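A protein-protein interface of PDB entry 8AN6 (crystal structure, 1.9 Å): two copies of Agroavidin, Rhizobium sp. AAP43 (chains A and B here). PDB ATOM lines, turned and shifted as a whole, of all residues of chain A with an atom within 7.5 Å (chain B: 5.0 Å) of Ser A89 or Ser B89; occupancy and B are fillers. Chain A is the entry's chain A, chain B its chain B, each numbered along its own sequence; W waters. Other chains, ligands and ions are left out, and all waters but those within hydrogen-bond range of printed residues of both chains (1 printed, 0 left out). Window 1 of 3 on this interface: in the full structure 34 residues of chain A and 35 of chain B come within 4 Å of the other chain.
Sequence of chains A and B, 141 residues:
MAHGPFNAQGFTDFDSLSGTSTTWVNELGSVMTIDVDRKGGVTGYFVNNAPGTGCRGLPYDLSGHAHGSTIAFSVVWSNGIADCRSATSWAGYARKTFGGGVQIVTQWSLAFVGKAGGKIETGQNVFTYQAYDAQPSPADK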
ATOM      1  N   SER A  63      13.916   8.528  13.678  1.00  0.00           N
ATOM      2  CA  SER A  63      13.721   8.353  15.135  1.00  0.00           C
ATOM      3  C   SER A  63      14.727   7.342  15.673  1.00  0.00           C
ATOM      4  O   SER A  63      15.156   6.401  14.926  1.00  0.00           O
ATOM      5  CB  SER A  63      12.273   8.006  15.474  1.00  0.00           C
ATOM      6  OG  SER A  63      11.910   6.735  14.954  1.00  0.00           O
ATOM      7  N   ILE A  71      24.501   4.692  19.501  1.00  0.00           N
ATOM      8  CA  ILE A  71      23.295   5.309  18.893  1.00  0.00           C
ATOM      9  C   ILE A  71      22.604   4.300  17.953  1.00  0.00           C
ATOM     10  O   ILE A  71      23.278   3.415  17.347  1.00  0.00           O
ATOM     11  CB  ILE A  71      23.670   6.610  18.181  1.00  0.00           C
ATOM     12  CG1 ILE A  71      22.421   7.309  17.661  1.00  0.00           C
ATOM     13  CG2 ILE A  71      24.685   6.385  17.066  1.00  0.00           C
ATOM     14  CD1 ILE A  71      22.673   8.759  17.321  1.00  0.00           C
ATOM     15  N   ALA A  72      21.286   4.383  17.878  1.00  0.00           N
ATOM     16  CA  ALA A  72      20.484   3.544  16.962  1.00  0.00           C
ATOM     17  C   ALA A  72      19.374   4.442  16.454  1.00  0.00           C
ATOM     18  O   ALA A  72      18.874   5.228  17.268  1.00  0.00           O
ATOM     19  CB  ALA A  72      19.978   2.304  17.654  1.00  0.00           C
ATOM     20  N   PHE A  73      19.091   4.397  15.153  1.00  0.00           N
ATOM     21  CA  PHE A  73      18.043   5.235  14.522  1.00  0.00           C
ATOM     22  C   PHE A  73      17.478   4.520  13.296  1.00  0.00           C
ATOM     23  O   PHE A  73      18.135   3.604  12.704  1.00  0.00           O
ATOM     24  CB  PHE A  73      18.558   6.635  14.184  1.00  0.00           C
ATOM     25  CG  PHE A  73      19.818   6.713  13.360  1.00  0.00           C
ATOM     26  CD1 PHE A  73      21.064   6.725  13.968  1.00  0.00           C
ATOM     27  CD2 PHE A  73      19.751   6.866  11.984  1.00  0.00           C
ATOM     28  CE1 PHE A  73      22.222   6.822  13.208  1.00  0.00           C
ATOM     29  CE2 PHE A  73      20.906   6.988  11.231  1.00  0.00           C
ATOM     30  CZ  PHE A  73      22.135   6.973  11.844  1.00  0.00           C
ATOM     31  N   SER A  74      16.291   4.962  12.905  1.00  0.00           N
ATOM     32  CA  SER A  74      15.409   4.298  11.920  1.00  0.00           C
ATOM     33  C   SER A  74      14.748   5.342  11.030  1.00  0.00           C
ATOM     34  O   SER A  74      14.439   6.443  11.538  1.00  0.00           O
ATOM     35  CB  SER A  74      14.376   3.463  12.620  1.00  0.00           C
ATOM     36  OG  SER A  74      15.012   2.508  13.431  1.00  0.00           O
ATOM     37  N   VAL A  75      14.618   5.010   9.744  1.00  0.00           N
ATOM     38  CA  VAL A  75      13.959   5.844   8.700  1.00  0.00           C
ATOM     39  C   VAL A  75      13.094   4.926   7.841  1.00  0.00           C
ATOM     40  O   VAL A  75      13.615   3.908   7.327  1.00  0.00           O
ATOM     41  CB  VAL A  75      14.999   6.600   7.860  1.00  0.00           C
ATOM     42  CG1 VAL A  75      14.359   7.351   6.695  1.00  0.00           C
ATOM     43  CG2 VAL A  75      15.776   7.557   8.737  1.00  0.00           C
ATOM     44  N   VAL A  76      11.795   5.191   7.783  1.00  0.00           N
ATOM     45  CA  VAL A  76      10.915   4.518   6.792  1.00  0.00           C
ATOM     46  C   VAL A  76      10.912   5.455   5.591  1.00  0.00           C
ATOM     47  O   VAL A  76      10.725   6.646   5.783  1.00  0.00           O
ATOM     48  CB  VAL A  76       9.491   4.229   7.296  1.00  0.00           C
ATOM     49  CG1 VAL A  76       8.555   3.943   6.127  1.00  0.00           C
ATOM     50  CG2 VAL A  76       9.474   3.057   8.267  1.00  0.00           C
ATOM     51  N   TRP A  77      11.180   4.922   4.417  1.00  0.00           N
ATOM     52  CA  TRP A  77      11.307   5.699   3.156  1.00  0.00           C
ATOM     53  C   TRP A  77       9.942   5.993   2.558  1.00  0.00           C
ATOM     54  O   TRP A  77       9.722   5.630   1.383  1.00  0.00           O
ATOM     55  CB  TRP A  77      12.187   4.908   2.188  1.00  0.00           C
ATOM     56  CG  TRP A  77      13.537   4.723   2.780  1.00  0.00           C
ATOM     57  CD1 TRP A  77      14.072   3.598   3.327  1.00  0.00           C
ATOM     58  CD2 TRP A  77      14.485   5.769   3.005  1.00  0.00           C
ATOM     59  NE1 TRP A  77      15.331   3.858   3.804  1.00  0.00           N
ATOM     60  CE2 TRP A  77      15.597   5.191   3.644  1.00  0.00           C
ATOM     61  CE3 TRP A  77      14.489   7.141   2.733  1.00  0.00           C
ATOM     62  CZ2 TRP A  77      16.729   5.932   3.959  1.00  0.00           C
ATOM     63  CZ3 TRP A  77      15.608   7.876   3.041  1.00  0.00           C
ATOM     64  CH2 TRP A  77      16.707   7.279   3.663  1.00  0.00           C
ATOM     65  N   ALA A  87      12.584   0.385   4.503  1.00  0.00           N
ATOM     66  CA  ALA A  87      12.927   0.957   5.827  1.00  0.00           C
ATOM     67  C   ALA A  87      14.371   0.639   6.118  1.00  0.00           C
ATOM     68  O   ALA A  87      14.832  -0.448   5.720  1.00  0.00           O
ATOM     69  CB  ALA A  87      12.015   0.418   6.895  1.00  0.00           C
ATOM     70  N   THR A  88      15.074   1.600   6.709  1.00  0.00           N
ATOM     71  CA  THR A  88      16.472   1.414   7.137  1.00  0.00           C
ATOM     72  C   THR A  88      16.582   1.704   8.633  1.00  0.00           C
ATOM     73  O   THR A  88      15.969   2.673   9.147  1.00  0.00           O
ATOM     74  CB  THR A  88      17.432   2.270   6.300  1.00  0.00           C
ATOM     75  OG1 THR A  88      17.182   1.961   4.930  1.00  0.00           O
ATOM     76  CG2 THR A  88      18.879   1.997   6.635  1.00  0.00           C
ATOM     77  N   SER A  89      17.367   0.897   9.317  1.00  0.00           N
ATOM     78  CA  SER A  89      17.799   1.176  10.700  1.00  0.00           C
ATOM     79  C   SER A  89      19.317   1.067  10.740  1.00  0.00           C
ATOM     80  O   SER A  89      19.886   0.219   9.992  1.00  0.00           O
ATOM     81  CB  SER A  89      17.128   0.238  11.630  1.00  0.00           C
ATOM     82  OG  SER A  89      17.631  -1.048  11.374  1.00  0.00           O
ATOM     83  N   TRP A  90      19.920   1.936  11.549  1.00  0.00           N
ATOM     84  CA  TRP A  90      21.371   2.065  11.787  1.00  0.00           C
ATOM     85  C   TRP A  90      21.613   1.849  13.279  1.00  0.00           C
ATOM     86  O   TRP A  90      20.773   2.294  14.053  1.00  0.00           O
ATOM     87  CB  TRP A  90      21.854   3.457  11.375  1.00  0.00           C
ATOM     88  CG  TRP A  90      21.912   3.780   9.910  1.00  0.00           C
ATOM     89  CD1 TRP A  90      23.022   3.761   9.117  1.00  0.00           C
ATOM     90  CD2 TRP A  90      20.852   4.291   9.089  1.00  0.00           C
ATOM     91  NE1 TRP A  90      22.715   4.184   7.850  1.00  0.00           N
ATOM     92  CE2 TRP A  90      21.398   4.537   7.811  1.00  0.00           C
ATOM     93  CE3 TRP A  90      19.501   4.576   9.318  1.00  0.00           C
ATOM     94  CZ2 TRP A  90      20.636   5.036   6.759  1.00  0.00           C
ATOM     95  CZ3 TRP A  90      18.759   5.096   8.285  1.00  0.00           C
ATOM     96  CH2 TRP A  90      19.317   5.303   7.022  1.00  0.00           C
ATOM     97  N   ALA A  91      22.665   1.127  13.647  1.00  0.00           N
ATOM     98  CA  ALA A  91      23.238   1.101  15.011  1.00  0.00           C
ATOM     99  C   ALA A  91      24.725   1.408  14.874  1.00  0.00           C
ATOM    100  O   ALA A  91      25.351   0.928  13.903  1.00  0.00           O
ATOM    101  CB  ALA A  91      23.002  -0.219  15.721  1.00  0.00           C
ATOM    102  N   GLY A  92      25.265   2.214  15.783  1.00  0.00           N
ATOM    103  CA  GLY A  92      26.609   2.785  15.587  1.00  0.00           C
ATOM    104  C   GLY A  92      27.274   3.168  16.883  1.00  0.00           C
ATOM    105  O   GLY A  92      26.586   3.262  17.927  1.00  0.00           O
ATOM    106  N   THR A 106      28.642   2.992  11.663  1.00  0.00           N
ATOM    107  CA  THR A 106      27.331   2.306  11.721  1.00  0.00           C
ATOM    108  C   THR A 106      27.288   1.062  10.844  1.00  0.00           C
ATOM    109  O   THR A 106      28.048   0.928   9.926  1.00  0.00           O
ATOM    110  CB  THR A 106      26.164   3.216  11.328  1.00  0.00           C
ATOM    111  OG1 THR A 106      26.217   3.467   9.921  1.00  0.00           O
ATOM    112  CG2 THR A 106      26.159   4.504  12.115  1.00  0.00           C
ATOM    113  N   GLN A 107      26.356   0.190  11.182  1.00  0.00           N
ATOM    114  CA  GLN A 107      25.854  -0.890  10.323  1.00  0.00           C
ATOM    115  C   GLN A 107      24.415  -0.526  10.036  1.00  0.00           C
ATOM    116  O   GLN A 107      23.718  -0.175  10.997  1.00  0.00           O
ATOM    117  CB  GLN A 107      25.937  -2.222  11.048  1.00  0.00           C
ATOM    118  CG  GLN A 107      25.407  -3.373  10.220  1.00  0.00           C
ATOM    119  CD  GLN A 107      26.482  -4.014   9.393  1.00  0.00           C
ATOM    120  OE1 GLN A 107      27.612  -3.533   9.309  1.00  0.00           O
ATOM    121  NE2 GLN A 107      26.121  -5.124   8.785  1.00  0.00           N
ATOM    122  N   TRP A 108      24.009  -0.600   8.776  1.00  0.00           N
ATOM    123  CA  TRP A 108      22.606  -0.366   8.369  1.00  0.00           C
ATOM    124  C   TRP A 108      22.057  -1.682   7.846  1.00  0.00           C
ATOM    125  O   TRP A 108      22.854  -2.525   7.365  1.00  0.00           O
ATOM    126  CB  TRP A 108      22.441   0.780   7.357  1.00  0.00           C
ATOM    127  CG  TRP A 108      23.250   0.675   6.107  1.00  0.00           C
ATOM    128  CD1 TRP A 108      24.469   1.236   5.891  1.00  0.00           C
ATOM    129  CD2 TRP A 108      22.914  -0.036   4.902  1.00  0.00           C
ATOM    130  NE1 TRP A 108      24.902   0.956   4.629  1.00  0.00           N
ATOM    131  CE2 TRP A 108      23.974   0.172   3.997  1.00  0.00           C
ATOM    132  CE3 TRP A 108      21.832  -0.828   4.499  1.00  0.00           C
ATOM    133  CZ2 TRP A 108      23.987  -0.370   2.713  1.00  0.00           C
ATOM    134  CZ3 TRP A 108      21.843  -1.364   3.229  1.00  0.00           C
ATOM    135  CH2 TRP A 108      22.908  -1.140   2.353  1.00  0.00           C
ATOM    136  N   SER A 109      20.752  -1.844   8.020  1.00  0.00           N
ATOM    137  CA  SER A 109      19.914  -2.904   7.409  1.00  0.00           C
ATOM    138  C   SER A 109      18.766  -2.229   6.666  1.00  0.00           C
ATOM    139  O   SER A 109      18.049  -1.438   7.311  1.00  0.00           O
ATOM    140  CB  SER A 109      19.383  -3.835   8.436  1.00  0.00           C
ATOM    141  OG  SER A 109      20.433  -4.418   9.144  1.00  0.00           O
ATOM    142  N   LEU A 110      18.612  -2.536   5.382  1.00  0.00           N
ATOM    143  CA  LEU A 110      17.529  -2.025   4.510  1.00  0.00           C
ATOM    144  C   LEU A 110      16.608  -3.200   4.164  1.00  0.00           C
ATOM    145  O   LEU A 110      17.087  -4.174   3.523  1.00  0.00           O
ATOM    146  CB  LEU A 110      18.173  -1.390   3.275  1.00  0.00           C
ATOM    147  CG  LEU A 110      17.257  -1.031   2.110  1.00  0.00           C
ATOM    148  CD1 LEU A 110      16.009  -0.295   2.558  1.00  0.00           C
ATOM    149  CD2 LEU A 110      18.037  -0.169   1.120  1.00  0.00           C
ATOM    150  N   ALA A 111      15.356  -3.104   4.601  1.00  0.00           N
ATOM    151  CA  ALA A 111      14.273  -4.069   4.331  1.00  0.00           C
ATOM    152  C   ALA A 111      13.374  -3.515   3.219  1.00  0.00           C
ATOM    153  O   ALA A 111      13.103  -2.301   3.209  1.00  0.00           O
ATOM    154  CB  ALA A 111      13.481  -4.324   5.580  1.00  0.00           C
ATOM    155  N   GLU A 121      19.024  -5.978   2.976  1.00  0.00           N
ATOM    156  CA  GLU A 121      20.418  -5.685   2.584  1.00  0.00           C
ATOM    157  C   GLU A 121      21.133  -5.046   3.769  1.00  0.00           C
ATOM    158  O   GLU A 121      20.464  -4.383   4.568  1.00  0.00           O
ATOM    159  CB  GLU A 121      20.483  -4.702   1.421  1.00  0.00           C
ATOM    160  CG  GLU A 121      20.030  -5.271   0.095  1.00  0.00           C
ATOM    161  CD  GLU A 121      20.171  -4.288  -1.057  1.00  0.00           C
ATOM    162  OE1 GLU A 121      20.728  -3.173  -0.839  1.00  0.00           O
ATOM    163  OE2 GLU A 121      19.724  -4.634  -2.160  1.00  0.00           O
ATOM    164  N   GLY A 123      24.933  -2.934   5.063  1.00  0.00           N
ATOM    165  CA  GLY A 123      26.224  -2.285   4.787  1.00  0.00           C
ATOM    166  C   GLY A 123      26.686  -1.473   5.960  1.00  0.00           C
ATOM    167  O   GLY A 123      26.070  -1.581   7.025  1.00  0.00           O
ATOM    168  N   ALA B  72      11.146  -0.410  10.867  1.00  0.00           N
ATOM    169  CA  ALA B  72      12.486  -0.225  11.458  1.00  0.00           C
ATOM    170  C   ALA B  72      12.299   0.419  12.823  1.00  0.00           C
ATOM    171  O   ALA B  72      11.444   1.299  12.949  1.00  0.00           O
ATOM    172  CB  ALA B  72      13.380   0.580  10.560  1.00  0.00           C
ATOM    173  N   PHE B  73      13.035  -0.059  13.815  1.00  0.00           N
ATOM    174  CA  PHE B  73      12.963   0.454  15.201  1.00  0.00           C
ATOM    175  C   PHE B  73      14.327   0.305  15.842  1.00  0.00           C
ATOM    176  O   PHE B  73      15.175  -0.529  15.399  1.00  0.00           O
ATOM    177  CB  PHE B  73      11.855  -0.241  15.995  1.00  0.00           C
ATOM    178  CG  PHE B  73      11.896  -1.751  16.038  1.00  0.00           C
ATOM    179  CD1 PHE B  73      11.216  -2.513  15.103  1.00  0.00           C
ATOM    180  CD2 PHE B  73      12.538  -2.403  17.082  1.00  0.00           C
ATOM    181  CE1 PHE B  73      11.226  -3.903  15.175  1.00  0.00           C
ATOM    182  CE2 PHE B  73      12.543  -3.789  17.154  1.00  0.00           C
ATOM    183  CZ  PHE B  73      11.874  -4.537  16.212  1.00  0.00           C
ATOM    184  N   SER B  74      14.516   1.117  16.876  1.00  0.00           N
ATOM    185  CA  SER B  74      15.815   1.351  17.543  1.00  0.00           C
ATOM    186  C   SER B  74      15.610   1.334  19.053  1.00  0.00           C
ATOM    187  O   SER B  74      14.562   1.794  19.509  1.00  0.00           O
ATOM    188  CB  SER B  74      16.431   2.643  17.096  1.00  0.00           C
ATOM    189  OG  SER B  74      16.625   2.632  15.700  1.00  0.00           O
ATOM    190  N   ALA B  87      23.752  -0.292  21.644  1.00  0.00           N
ATOM    191  CA  ALA B  87      22.491   0.106  20.976  1.00  0.00           C
ATOM    192  C   ALA B  87      22.243  -0.897  19.862  1.00  0.00           C
ATOM    193  O   ALA B  87      23.255  -1.436  19.292  1.00  0.00           O
ATOM    194  CB  ALA B  87      22.559   1.519  20.454  1.00  0.00           C
ATOM    195  N   THR B  88      20.964  -1.193  19.653  1.00  0.00           N
ATOM    196  CA  THR B  88      20.469  -2.133  18.634  1.00  0.00           C
ATOM    197  C   THR B  88      19.434  -1.439  17.758  1.00  0.00           C
ATOM    198  O   THR B  88      18.530  -0.731  18.293  1.00  0.00           O
ATOM    199  CB  THR B  88      19.908  -3.407  19.267  1.00  0.00           C
ATOM    200  OG1 THR B  88      20.884  -3.900  20.187  1.00  0.00           O
ATOM    201  CG2 THR B  88      19.633  -4.470  18.227  1.00  0.00           C
ATOM    202  N   SER B  89      19.524  -1.686  16.464  1.00  0.00           N
ATOM    203  CA  SER B  89      18.485  -1.311  15.478  1.00  0.00           C
ATOM    204  C   SER B  89      18.063  -2.550  14.700  1.00  0.00           C
ATOM    205  O   SER B  89      18.915  -3.431  14.456  1.00  0.00           O
ATOM    206  CB  SER B  89      18.994  -0.260  14.568  1.00  0.00           C
ATOM    207  OG  SER B  89      20.141  -0.752  13.900  1.00  0.00           O
ATOM    208  N   TRP B  90      16.777  -2.627  14.393  1.00  0.00           N
ATOM    209  CA  TRP B  90      16.146  -3.717  13.615  1.00  0.00           C
ATOM    210  C   TRP B  90      15.550  -3.098  12.347  1.00  0.00           C
ATOM    211  O   TRP B  90      14.898  -2.066  12.463  1.00  0.00           O
ATOM    212  CB  TRP B  90      15.049  -4.396  14.439  1.00  0.00           C
ATOM    213  CG  TRP B  90      15.494  -5.210  15.618  1.00  0.00           C
ATOM    214  CD1 TRP B  90      15.572  -6.572  15.656  1.00  0.00           C
ATOM    215  CD2 TRP B  90      15.799  -4.752  16.943  1.00  0.00           C
ATOM    216  NE1 TRP B  90      15.976  -6.991  16.889  1.00  0.00           N
ATOM    217  CE2 TRP B  90      16.096  -5.896  17.710  1.00  0.00           C
ATOM    218  CE3 TRP B  90      15.873  -3.491  17.560  1.00  0.00           C
ATOM    219  CZ2 TRP B  90      16.473  -5.815  19.051  1.00  0.00           C
ATOM    220  CZ3 TRP B  90      16.246  -3.416  18.883  1.00  0.00           C
ATOM    221  CH2 TRP B  90      16.540  -4.561  19.621  1.00  0.00           C
ATOM    222  N   ALA B  91      15.665  -3.757  11.206  1.00  0.00           N
ATOM    223  CA  ALA B  91      14.834  -3.425  10.029  1.00  0.00           C
ATOM    224  C   ALA B  91      14.256  -4.729   9.503  1.00  0.00           C
ATOM    225  O   ALA B  91      14.947  -5.746   9.530  1.00  0.00           O
ATOM    226  CB  ALA B  91      15.636  -2.673   8.998  1.00  0.00           C
ATOM    227  N   GLN B 107      16.527  -8.054  10.566  1.00  0.00           N
ATOM    228  CA  GLN B 107      17.990  -8.068  10.764  1.00  0.00           C
ATOM    229  C   GLN B 107      18.276  -7.018  11.828  1.00  0.00           C
ATOM    230  O   GLN B 107      17.710  -5.929  11.700  1.00  0.00           O
ATOM    231  CB  GLN B 107      18.725  -7.716   9.476  1.00  0.00           C
ATOM    232  CG  GLN B 107      20.237  -7.654   9.639  1.00  0.00           C
ATOM    233  CD  GLN B 107      20.919  -8.911   9.162  1.00  0.00           C
ATOM    234  OE1 GLN B 107      20.338  -9.725   8.454  1.00  0.00           O
ATOM    235  NE2 GLN B 107      22.165  -9.087   9.571  1.00  0.00           N
ATOM    236  N   TRP B 108      19.065  -7.364  12.850  1.00  0.00           N
ATOM    237  CA  TRP B 108      19.523  -6.403  13.878  1.00  0.00           C
ATOM    238  C   TRP B 108      21.025  -6.149  13.728  1.00  0.00           C
ATOM    239  O   TRP B 108      21.739  -7.035  13.222  1.00  0.00           O
ATOM    240  CB  TRP B 108      19.175  -6.860  15.296  1.00  0.00           C
ATOM    241  CG  TRP B 108      19.635  -8.232  15.666  1.00  0.00           C
ATOM    242  CD1 TRP B 108      18.909  -9.385  15.603  1.00  0.00           C
ATOM    243  CD2 TRP B 108      20.926  -8.601  16.181  1.00  0.00           C
ATOM    244  NE1 TRP B 108      19.662 -10.443  16.039  1.00  0.00           N
ATOM    245  CE2 TRP B 108      20.902  -9.997  16.395  1.00  0.00           C
ATOM    246  CE3 TRP B 108      22.095  -7.895  16.476  1.00  0.00           C
ATOM    247  CZ2 TRP B 108      21.995 -10.693  16.900  1.00  0.00           C
ATOM    248  CZ3 TRP B 108      23.183  -8.588  16.964  1.00  0.00           C
ATOM    249  CH2 TRP B 108      23.131  -9.966  17.172  1.00  0.00           C
ATOM    250  N   SER B 109      21.430  -4.935  14.094  1.00  0.00           N
ATOM    251  CA  SER B 109      22.829  -4.538  14.352  1.00  0.00           C
ATOM    252  C   SER B 109      22.904  -4.051  15.788  1.00  0.00           C
ATOM    253  O   SER B 109      22.007  -3.275  16.192  1.00  0.00           O
ATOM    254  CB  SER B 109      23.288  -3.480  13.384  1.00  0.00           C
ATOM    255  OG  SER B 109      22.904  -3.809  12.064  1.00  0.00           O
HETATM  256  O   HOH W   1      19.603  -3.585  11.542  1.00  0.00           O
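The backbone carbonyl oxygen of Trp A90 sits close to the side-chain hydroxyl of Ser B89, at 3.1 Å.
The side-chain hydroxyl (OG) of Ser A74 lies within hydrogen-bond range of the backbone NH (N) of Phe B73 (3.3 Å).
The side-chain hydroxyl of Ser A89 sits at hydrogen-bond distance from the backbone NH of Ala B91 (3.4 Å).
The side-chain hydroxyl (OG) of Ser A74 is in hydrogen-bond range of the side-chain hydroxyl (OG) of Ser B74.
The backbone NH (N) of Ala A91 lies within hydrogen-bond range of the side-chain hydroxyl (OG) of Ser B89, at 3.2 Å.
The side-chain hydroxyl of Ser B74 sits at hydrogen-bond distance from the backbone NH of Phe A73.
The side-chain hydroxyl (OG) of Ser A89 sits close to the backbone carbonyl oxygen (O) of Trp B90.
The backbone carbonyl oxygen (O) of Ala A91 lies within hydrogen-bond range of the backbone NH (N) of Gln A107, at 3.0 Å.
The backbone NH of Ser A74 is in hydrogen-bond range of the backbone carbonyl oxygen of Ser A63, 2.7 Å away.
The backbone carbonyl oxygen (O) of Phe A73 is in hydrogen-bond range of the backbone NH (N) of Trp A90 (2.7 Å).
O of Ser A89 sits at hydrogen-bond distance from N of Ser A109, at 3.0 Å.
The backbone carbonyl oxygen (O) of Ile A71 is in hydrogen-bond range of the backbone NH (N) of Gly A92, 2.8 Å away.
O of Thr A88 is in hydrogen-bond range of N of Val A75 (2.8 Å).
CB of Ala B87 touches O of Ile A71 (3.7 Å).
Ala A72 touches Ser B74.
OG of Ser A74 touches C of Ala B72, at 3.5 Å.
Ala A87 touches Ala B72 (CB to CB, 3.9 Å).
Thr A88 touches Ala B72.
Ser A89 touches Ala B72.
CB of Ser A89 touches CB of Ser B89 (3.5 Å).
OG of Ser B109 touches CG of Gln A107, at 3.1 Å.
Ala B91 touches Ser A109.
Ser B109 touches Ser A109.
Of chain B, only Ala B72, Ser B89, Trp B90 and Ala B91 come within 4 Å of Ser A89.
Of chain A, only Ser A89, Trp A90 and Ala A91 come within 4 Å of Ser B89.
Printed residues of chain B within 4 Å of Ser A74: Ala B72, Phe B73 and Ser B74.
Printed residues of chain B within 4 Å of Gln A107: Ser B109 (3.1 Å).
Of the printed residues of chain A, Phe B73 touches Ser A74 (3.3 Å).
Printed residues of chain A within 4 Å of Ala B72: Ser A74 (3.5 Å), Ala A87 (3.9 Å), Thr A88 (3.6 Å) and Ser A89 (3.9 Å).
Of the printed residues of chain B, Trp A90 touches Ser B89 (3.1 Å).
The nearest residue of chain B that does not touch Ser A89 is Phe B73 (4.3 Å).
The nearest residue of chain A that does not touch Ser B89 is Ala A72 (4.1 Å).
The nearest printed residue of chain B that does not touch Ala A91 is Thr B88 (4.3 Å).
Hydrophobic or aromatic side chains of chain A within 4 Å of the printed part of chain B: Ala A72, Ala A87 and Ala A91.
Hydrophobic or aromatic side chains of chain B within 4 Å of the printed part of chain A: Ala B72, Ala B87 and Ala B91.
Among the printed residues, no Asp or Glu carboxylate lies within 4 Å of a Lys or Arg side-chain nitrogen of the other chain.
Ala A72 touches Ala B87, and with the chains exchanged Ala A87 touches Ala B72.
Ala A72 touches Thr B88, and with the chains exchanged Thr A88 touches Ala B72.
Ala A91 touches Ser B109, and with the chains exchanged Ser A109 touches Ala B91.
Gln A107 touches Ser B109, and with the chains exchanged Ser A109 touches Gln B107.
Of the 22 pairs that touch across the chains among the printed residues, 19 have their exchanged pair printed and touching as well.
Water W1 lies within hydrogen-bond range of OG of Ser A109, O of Ser B89, O of Gln B107, OG of Ser A89 and OG of Ser B109.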
